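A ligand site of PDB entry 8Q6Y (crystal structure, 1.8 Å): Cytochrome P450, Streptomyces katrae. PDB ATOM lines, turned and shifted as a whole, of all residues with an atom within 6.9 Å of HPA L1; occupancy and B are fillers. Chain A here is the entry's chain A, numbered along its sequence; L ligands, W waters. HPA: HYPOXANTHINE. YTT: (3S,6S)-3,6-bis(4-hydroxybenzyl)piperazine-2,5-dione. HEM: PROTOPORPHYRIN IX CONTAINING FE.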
ATOM      1  N   GLN A  72       6.087 -13.522  29.690  1.00  0.00           N
ATOM      2  CA  GLN A  72       5.878 -12.583  28.565  1.00  0.00           C
ATOM      3  C   GLN A  72       5.217 -11.295  29.079  1.00  0.00           C
ATOM      4  O   GLN A  72       5.582 -10.215  28.616  1.00  0.00           O
ATOM      5  CB  GLN A  72       4.998 -13.284  27.535  1.00  0.00           C
ATOM      6  CG  GLN A  72       5.027 -12.557  26.238  1.00  0.00           C
ATOM      7  CD  GLN A  72       4.193 -13.153  25.135  1.00  0.00           C
ATOM      8  OE1 GLN A  72       4.254 -12.638  24.029  1.00  0.00           O
ATOM      9  NE2 GLN A  72       3.442 -14.222  25.419  1.00  0.00           N
ATOM     10  N   TYR A  73       4.244 -11.431  29.974  1.00  0.00           N
ATOM     11  CA  TYR A  73       3.482 -10.341  30.611  1.00  0.00           C
ATOM     12  C   TYR A  73       2.768 -10.934  31.809  1.00  0.00           C
ATOM     13  O   TYR A  73       2.811 -12.154  31.998  1.00  0.00           O
ATOM     14  CB  TYR A  73       2.497  -9.713  29.620  1.00  0.00           C
ATOM     15  CG  TYR A  73       1.731 -10.712  28.782  1.00  0.00           C
ATOM     16  CD1 TYR A  73       0.692 -11.460  29.311  1.00  0.00           C
ATOM     17  CD2 TYR A  73       2.021 -10.853  27.426  1.00  0.00           C
ATOM     18  CE1 TYR A  73       0.014 -12.393  28.532  1.00  0.00           C
ATOM     19  CE2 TYR A  73       1.348 -11.777  26.638  1.00  0.00           C
ATOM     20  CZ  TYR A  73       0.340 -12.542  27.189  1.00  0.00           C
ATOM     21  OH  TYR A  73      -0.364 -13.389  26.377  1.00  0.00           O
ATOM     22  N   PHE A 167      -7.434  -9.593  28.266  1.00  0.00           N
ATOM     23  CA  PHE A 167      -6.404  -9.942  27.265  1.00  0.00           C
ATOM     24  C   PHE A 167      -5.344  -8.830  27.194  1.00  0.00           C
ATOM     25  O   PHE A 167      -4.635  -8.777  26.210  1.00  0.00           O
ATOM     26  CB  PHE A 167      -7.086 -10.216  25.935  1.00  0.00           C
ATOM     27  CG  PHE A 167      -7.844 -11.505  26.036  1.00  0.00           C
ATOM     28  CD1 PHE A 167      -7.168 -12.711  25.969  1.00  0.00           C
ATOM     29  CD2 PHE A 167      -9.212 -11.510  26.298  1.00  0.00           C
ATOM     30  CE1 PHE A 167      -7.833 -13.897  26.193  1.00  0.00           C
ATOM     31  CE2 PHE A 167      -9.892 -12.713  26.465  1.00  0.00           C
ATOM     32  CZ  PHE A 167      -9.194 -13.902  26.405  1.00  0.00           C
ATOM     33  N   ASN A 169      -1.755  -7.294  27.864  1.00  0.00           N
ATOM     34  CA  ASN A 169      -0.354  -7.729  28.037  1.00  0.00           C
ATOM     35  C   ASN A 169       0.355  -6.638  28.841  1.00  0.00           C
ATOM     36  O   ASN A 169       0.890  -5.718  28.212  1.00  0.00           O
ATOM     37  CB  ASN A 169       0.307  -7.967  26.679  1.00  0.00           C
ATOM     38  CG  ASN A 169      -0.268  -9.101  25.871  1.00  0.00           C
ATOM     39  OD1 ASN A 169       0.093  -9.217  24.688  1.00  0.00           O
ATOM     40  ND2 ASN A 169      -1.120  -9.944  26.460  1.00  0.00           N
ATOM     41  N   ALA A 230     -11.987 -16.486  25.267  1.00  0.00           N
ATOM     42  CA  ALA A 230     -11.040 -16.912  24.219  1.00  0.00           C
ATOM     43  C   ALA A 230     -11.769 -16.892  22.869  1.00  0.00           C
ATOM     44  O   ALA A 230     -11.162 -16.436  21.894  1.00  0.00           O
ATOM     45  CB  ALA A 230     -10.437 -18.253  24.525  1.00  0.00           C
ATOM     46  N   ILE A 233     -12.671 -12.996  21.756  1.00  0.00           N
ATOM     47  CA  ILE A 233     -11.502 -12.132  21.437  1.00  0.00           C
ATOM     48  C   ILE A 233     -10.856 -12.592  20.126  1.00  0.00           C
ATOM     49  O   ILE A 233     -10.460 -11.715  19.354  1.00  0.00           O
ATOM     50  CB  ILE A 233     -10.482 -12.037  22.576  1.00  0.00           C
ATOM     51  CG1 ILE A 233      -9.698 -10.733  22.473  1.00  0.00           C
ATOM     52  CG2 ILE A 233      -9.541 -13.202  22.664  1.00  0.00           C
ATOM     53  CD1 ILE A 233     -10.565  -9.526  22.738  1.00  0.00           C
ATOM     54  N   SER A 234     -10.824 -13.904  19.848  1.00  0.00           N
ATOM     55  CA  SER A 234     -10.133 -14.464  18.663  1.00  0.00           C
ATOM     56  C   SER A 234     -11.024 -14.276  17.428  1.00  0.00           C
ATOM     57  O   SER A 234     -10.496 -13.916  16.356  1.00  0.00           O
ATOM     58  CB  SER A 234      -9.724 -15.892  18.926  1.00  0.00           C
ATOM     59  OG  SER A 234      -8.605 -15.902  19.797  1.00  0.00           O
ATOM     60  N   SER A 276      -3.586  -9.999  13.479  1.00  0.00           N
ATOM     61  CA  SER A 276      -4.280  -9.825  14.776  1.00  0.00           C
ATOM     62  C   SER A 276      -3.441 -10.328  15.964  1.00  0.00           C
ATOM     63  O   SER A 276      -3.644  -9.782  17.077  1.00  0.00           O
ATOM     64  CB  SER A 276      -5.636 -10.407  14.772  1.00  0.00           C
ATOM     65  OG  SER A 276      -5.512 -11.778  14.688  1.00  0.00           O
ATOM     66  N   ILE A 277      -2.498 -11.235  15.818  1.00  0.00           N
ATOM     67  CA  ILE A 277      -1.716 -11.738  16.986  1.00  0.00           C
ATOM     68  C   ILE A 277      -0.646 -10.725  17.347  1.00  0.00           C
ATOM     69  O   ILE A 277       0.220 -10.459  16.515  1.00  0.00           O
ATOM     70  CB  ILE A 277      -1.104 -13.143  16.757  1.00  0.00           C
ATOM     71  CG1 ILE A 277      -2.196 -14.175  16.538  1.00  0.00           C
ATOM     72  CG2 ILE A 277      -0.219 -13.513  17.945  1.00  0.00           C
ATOM     73  CD1 ILE A 277      -1.673 -15.594  16.278  1.00  0.00           C
ATOM     74  N   GLY A 278      -0.767 -10.123  18.529  1.00  0.00           N
ATOM     75  CA  GLY A 278       0.130  -9.030  18.931  1.00  0.00           C
ATOM     76  C   GLY A 278       1.173  -9.465  19.944  1.00  0.00           C
ATOM     77  O   GLY A 278       1.844  -8.598  20.500  1.00  0.00           O
ATOM     78  N   ASP A 279       1.243 -10.752  20.262  1.00  0.00           N
ATOM     79  CA  ASP A 279       2.231 -11.289  21.228  1.00  0.00           C
ATOM     80  C   ASP A 279       2.797 -12.578  20.617  1.00  0.00           C
ATOM     81  O   ASP A 279       2.685 -12.762  19.398  1.00  0.00           O
ATOM     82  CB  ASP A 279       1.566 -11.507  22.575  1.00  0.00           C
ATOM     83  CG  ASP A 279       0.513 -12.578  22.498  1.00  0.00           C
ATOM     84  OD1 ASP A 279       0.124 -12.917  21.338  1.00  0.00           O
ATOM     85  OD2 ASP A 279       0.088 -13.099  23.562  1.00  0.00           O
ATOM     86  N   GLY A 280       3.443 -13.397  21.434  1.00  0.00           N
ATOM     87  CA  GLY A 280       3.971 -14.713  21.033  1.00  0.00           C
ATOM     88  C   GLY A 280       3.127 -15.792  21.657  1.00  0.00           C
ATOM     89  O   GLY A 280       2.476 -15.520  22.678  1.00  0.00           O
ATOM     90  N   LEU A 281       3.152 -16.996  21.096  1.00  0.00           N
ATOM     91  CA  LEU A 281       2.573 -18.154  21.784  1.00  0.00           C
ATOM     92  C   LEU A 281       3.634 -18.663  22.743  1.00  0.00           C
ATOM     93  O   LEU A 281       4.736 -18.994  22.329  1.00  0.00           O
ATOM     94  CB  LEU A 281       2.179 -19.215  20.750  1.00  0.00           C
ATOM     95  CG  LEU A 281       1.284 -18.753  19.608  1.00  0.00           C
ATOM     96  CD1 LEU A 281       0.818 -19.978  18.779  1.00  0.00           C
ATOM     97  CD2 LEU A 281       0.117 -17.976  20.159  1.00  0.00           C
ATOM     98  N   PRO A 282       3.388 -18.640  24.066  1.00  0.00           N
ATOM     99  CA  PRO A 282       4.422 -18.972  25.039  1.00  0.00           C
ATOM    100  C   PRO A 282       4.548 -20.471  25.302  1.00  0.00           C
ATOM    101  O   PRO A 282       3.574 -21.193  25.333  1.00  0.00           O
ATOM    102  CB  PRO A 282       3.928 -18.234  26.307  1.00  0.00           C
ATOM    103  CG  PRO A 282       2.438 -18.313  26.211  1.00  0.00           C
ATOM    104  CD  PRO A 282       2.140 -18.196  24.732  1.00  0.00           C
ATOM    105  N   SER A 334      -1.895 -19.584  12.226  1.00  0.00           N
ATOM    106  CA  SER A 334      -2.807 -18.609  12.890  1.00  0.00           C
ATOM    107  C   SER A 334      -3.756 -19.340  13.863  1.00  0.00           C
ATOM    108  O   SER A 334      -4.421 -18.676  14.670  1.00  0.00           O
ATOM    109  CB  SER A 334      -3.582 -17.836  11.871  1.00  0.00           C
ATOM    110  OG  SER A 334      -2.717 -16.952  11.147  1.00  0.00           O
ATOM    111  N   MET A 382      -3.178  -8.317  23.836  1.00  0.00           N
ATOM    112  CA  MET A 382      -2.817  -9.590  23.173  1.00  0.00           C
ATOM    113  C   MET A 382      -3.037  -9.496  21.648  1.00  0.00           C
ATOM    114  O   MET A 382      -2.325 -10.230  20.914  1.00  0.00           O
ATOM    115  CB  MET A 382      -3.635 -10.774  23.704  1.00  0.00           C
ATOM    116  CG  MET A 382      -3.165 -12.057  23.155  1.00  0.00           C
ATOM    117  SD  MET A 382      -3.971 -13.461  23.987  1.00  0.00           S
ATOM    118  CE  MET A 382      -5.556 -13.521  23.146  1.00  0.00           C
ATOM    119  N   LYS A 383      -4.054  -8.759  21.193  1.00  0.00           N
ATOM    120  CA  LYS A 383      -4.407  -8.694  19.750  1.00  0.00           C
ATOM    121  C   LYS A 383      -3.989  -7.337  19.219  1.00  0.00           C
ATOM    122  O   LYS A 383      -4.079  -6.389  20.013  1.00  0.00           O
ATOM    123  CB  LYS A 383      -5.908  -8.901  19.529  1.00  0.00           C
ATOM    124  CG  LYS A 383      -6.453 -10.254  19.995  1.00  0.00           C
ATOM    125  CD  LYS A 383      -5.808 -11.414  19.289  1.00  0.00           C
ATOM    126  CE  LYS A 383      -6.547 -12.728  19.503  1.00  0.00           C
ATOM    127  NZ  LYS A 383      -5.804 -13.898  18.970  1.00  0.00           N
HETATM  128  N1  HPA L   1      -1.827 -14.847  21.431  1.00  0.00           N
HETATM  129  C2  HPA L   1      -1.478 -15.787  22.319  1.00  0.00           C
HETATM  130  N3  HPA L   1      -2.191 -16.842  22.563  1.00  0.00           N
HETATM  131  C4  HPA L   1      -3.348 -16.971  21.876  1.00  0.00           C
HETATM  132  C5  HPA L   1      -3.785 -16.025  20.935  1.00  0.00           C
HETATM  133  C6  HPA L   1      -2.995 -14.861  20.682  1.00  0.00           C
HETATM  134  O6  HPA L   1      -3.254 -13.949  19.890  1.00  0.00           O
HETATM  135  N7  HPA L   1      -4.987 -16.495  20.471  1.00  0.00           N
HETATM  136  C8  HPA L   1      -5.226 -17.641  21.119  1.00  0.00           C
HETATM  137  N9  HPA L   1      -4.273 -17.987  21.980  1.00  0.00           N
HETATM  138  OB  YTT L   2      -8.385 -21.325  27.416  1.00  0.00           O
HETATM  139  CB  YTT L   2      -7.339 -20.786  27.780  1.00  0.00           C
HETATM  140  CAB YTT L   2      -7.400 -19.446  28.513  1.00  0.00           C
HETATM  141  CBB YTT L   2      -8.081 -18.366  27.629  1.00  0.00           C
HETATM  142  CGB YTT L   2      -8.551 -17.188  28.428  1.00  0.00           C
HETATM  143  CD3 YTT L   2      -7.656 -16.227  28.889  1.00  0.00           C
HETATM  144  CE3 YTT L   2      -8.084 -15.168  29.687  1.00  0.00           C
HETATM  145  CZB YTT L   2      -9.426 -15.026  29.983  1.00  0.00           C
HETATM  146  OHB YTT L   2      -9.841 -13.989  30.765  1.00  0.00           O
HETATM  147  CE4 YTT L   2     -10.333 -15.965  29.537  1.00  0.00           C
HETATM  148  CD4 YTT L   2      -9.887 -17.027  28.746  1.00  0.00           C
HETATM  149  NB  YTT L   2      -6.092 -18.995  28.973  1.00  0.00           N
HETATM  150  NA  YTT L   2      -6.152 -21.328  27.564  1.00  0.00           N
HETATM  151  CAA YTT L   2      -4.848 -20.710  27.761  1.00  0.00           C
HETATM  152  CA  YTT L   2      -4.901 -19.486  28.651  1.00  0.00           C
HETATM  153  OA  YTT L   2      -3.842 -18.980  29.053  1.00  0.00           O
HETATM  154  CBA YTT L   2      -4.193 -20.317  26.413  1.00  0.00           C
HETATM  155  CGA YTT L   2      -5.012 -19.336  25.623  1.00  0.00           C
HETATM  156  CD2 YTT L   2      -4.777 -17.967  25.695  1.00  0.00           C
HETATM  157  CE2 YTT L   2      -5.545 -17.077  24.959  1.00  0.00           C
HETATM  158  CZA YTT L   2      -6.579 -17.521  24.160  1.00  0.00           C
HETATM  159  OHA YTT L   2      -7.357 -16.639  23.443  1.00  0.00           O
HETATM  160  CE1 YTT L   2      -6.829 -18.877  24.072  1.00  0.00           C
HETATM  161  CD1 YTT L   2      -6.051 -19.768  24.811  1.00  0.00           C
HETATM  162  CHA HEM L   3      -6.050 -22.017  21.266  1.00  0.00           C
HETATM  163  CHB HEM L   3      -6.454 -18.909  17.532  1.00  0.00           C
HETATM  164  CHC HEM L   3     -11.275 -19.233  17.666  1.00  0.00           C
HETATM  165  CHD HEM L   3     -10.786 -21.501  21.953  1.00  0.00           C
HETATM  166  C1A HEM L   3      -5.760 -21.188  20.194  1.00  0.00           C
HETATM  167  C2A HEM L   3      -4.474 -20.871  19.751  1.00  0.00           C
HETATM  168  C3A HEM L   3      -4.596 -20.010  18.702  1.00  0.00           C
HETATM  169  C4A HEM L   3      -5.958 -19.755  18.509  1.00  0.00           C
HETATM  170  CMA HEM L   3      -3.500 -19.389  17.892  1.00  0.00           C
HETATM  171  CAA HEM L   3      -3.144 -21.430  20.234  1.00  0.00           C
HETATM  172  CBA HEM L   3      -2.558 -20.823  21.494  1.00  0.00           C
HETATM  173  CGA HEM L   3      -1.230 -21.450  21.799  1.00  0.00           C
HETATM  174  O1A HEM L   3      -0.551 -21.069  22.805  1.00  0.00           O
HETATM  175  O2A HEM L   3      -0.774 -22.362  21.057  1.00  0.00           O
HETATM  176  C1B HEM L   3      -7.802 -18.705  17.218  1.00  0.00           C
HETATM  177  C2B HEM L   3      -8.283 -17.932  16.132  1.00  0.00           C
HETATM  178  C3B HEM L   3      -9.651 -18.035  16.165  1.00  0.00           C
HETATM  179  C4B HEM L   3      -9.966 -18.901  17.315  1.00  0.00           C
HETATM  180  CMB HEM L   3      -7.492 -17.112  15.131  1.00  0.00           C
HETATM  181  CAB HEM L   3     -10.740 -17.523  15.345  1.00  0.00           C
HETATM  182  CBB HEM L   3     -10.558 -17.028  14.134  1.00  0.00           C
HETATM  183  C1C HEM L   3     -11.581 -19.869  18.882  1.00  0.00           C
HETATM  184  C2C HEM L   3     -12.834 -20.081  19.407  1.00  0.00           C
HETATM  185  C3C HEM L   3     -12.684 -20.696  20.623  1.00  0.00           C
HETATM  186  C4C HEM L   3     -11.293 -20.835  20.853  1.00  0.00           C
HETATM  187  CMC HEM L   3     -14.160 -19.713  18.754  1.00  0.00           C
HETATM  188  CAC HEM L   3     -13.709 -21.139  21.599  1.00  0.00           C
HETATM  189  CBC HEM L   3     -15.039 -20.982  21.506  1.00  0.00           C
HETATM  190  C1D HEM L   3      -9.445 -21.854  22.123  1.00  0.00           C
HETATM  191  C2D HEM L   3      -8.902 -22.579  23.271  1.00  0.00           C
HETATM  192  C3D HEM L   3      -7.594 -22.737  23.091  1.00  0.00           C
HETATM  193  C4D HEM L   3      -7.332 -22.092  21.795  1.00  0.00           C
HETATM  194  CMD HEM L   3      -9.642 -23.087  24.498  1.00  0.00           C
HETATM  195  CAD HEM L   3      -6.605 -23.436  24.002  1.00  0.00           C
HETATM  196  CBD HEM L   3      -6.326 -24.837  23.411  1.00  0.00           C
HETATM  197  CGD HEM L   3      -5.251 -25.658  24.082  1.00  0.00           C
HETATM  198  O1D HEM L   3      -5.022 -26.862  23.730  1.00  0.00           O
HETATM  199  O2D HEM L   3      -4.563 -25.196  25.013  1.00  0.00           O
HETATM  200  NA  HEM L   3      -6.657 -20.499  19.444  1.00  0.00           N
HETATM  201  NB  HEM L   3      -8.830 -19.264  17.869  1.00  0.00           N
HETATM  202  NC  HEM L   3     -10.638 -20.365  19.725  1.00  0.00           N
HETATM  203  ND  HEM L   3      -8.474 -21.597  21.264  1.00  0.00           N
HETATM  204 FE   HEM L   3      -8.658 -20.641  19.447  1.00  0.00          FE
HETATM  205  O   HOH W   1      -1.693 -19.030  24.198  1.00  0.00           O
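The side-chain amino group (NZ) of Lys 383 is in hydrogen-bond range of an oxygen (O6) of HPA L1 (2.7 Å). OD1 of Asp 279 lies within hydrogen-bond range of N1 of HPA L1, 2.7 Å away. SD of Met 382 sits close to N1 of HPA L1 (3.6 Å).
OD2 of Asp 279 lies within hydrogen-bond range of OH of Tyr 73, at 2.9 Å. O of Met 382 sits at hydrogen-bond distance from N of Gly 278 (2.9 Å). The side-chain amide oxygen (OD1) of Asn 169 sits close to the backbone NH (N) of Met 382, 3.5 Å away. The backbone NH of Met 382 is in hydrogen-bond range of the backbone carbonyl oxygen of Phe 167, at 2.8 Å. The side-chain hydroxyl (OG) of Ser 234 lies close to the backbone carbonyl oxygen (O) of Ala 230, at 3.3 Å. The backbone NH (N) of Gly 280 is in hydrogen-bond range of the side-chain amide oxygen (OE1) of Gln 72, at 2.8 Å.
Residues that only touch HPA L1: Ser 234, Ile 277, Gly 280 and Leu 281. Hydrophobic or aromatic side chains that line HPA L1: Ile 277, Leu 281 and Met 382.
Water W1 bridges an oxygen (O1A) of HEM L3 (2.7 Å) and a nitrogen (N3) of HPA L1 (2.8 Å).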
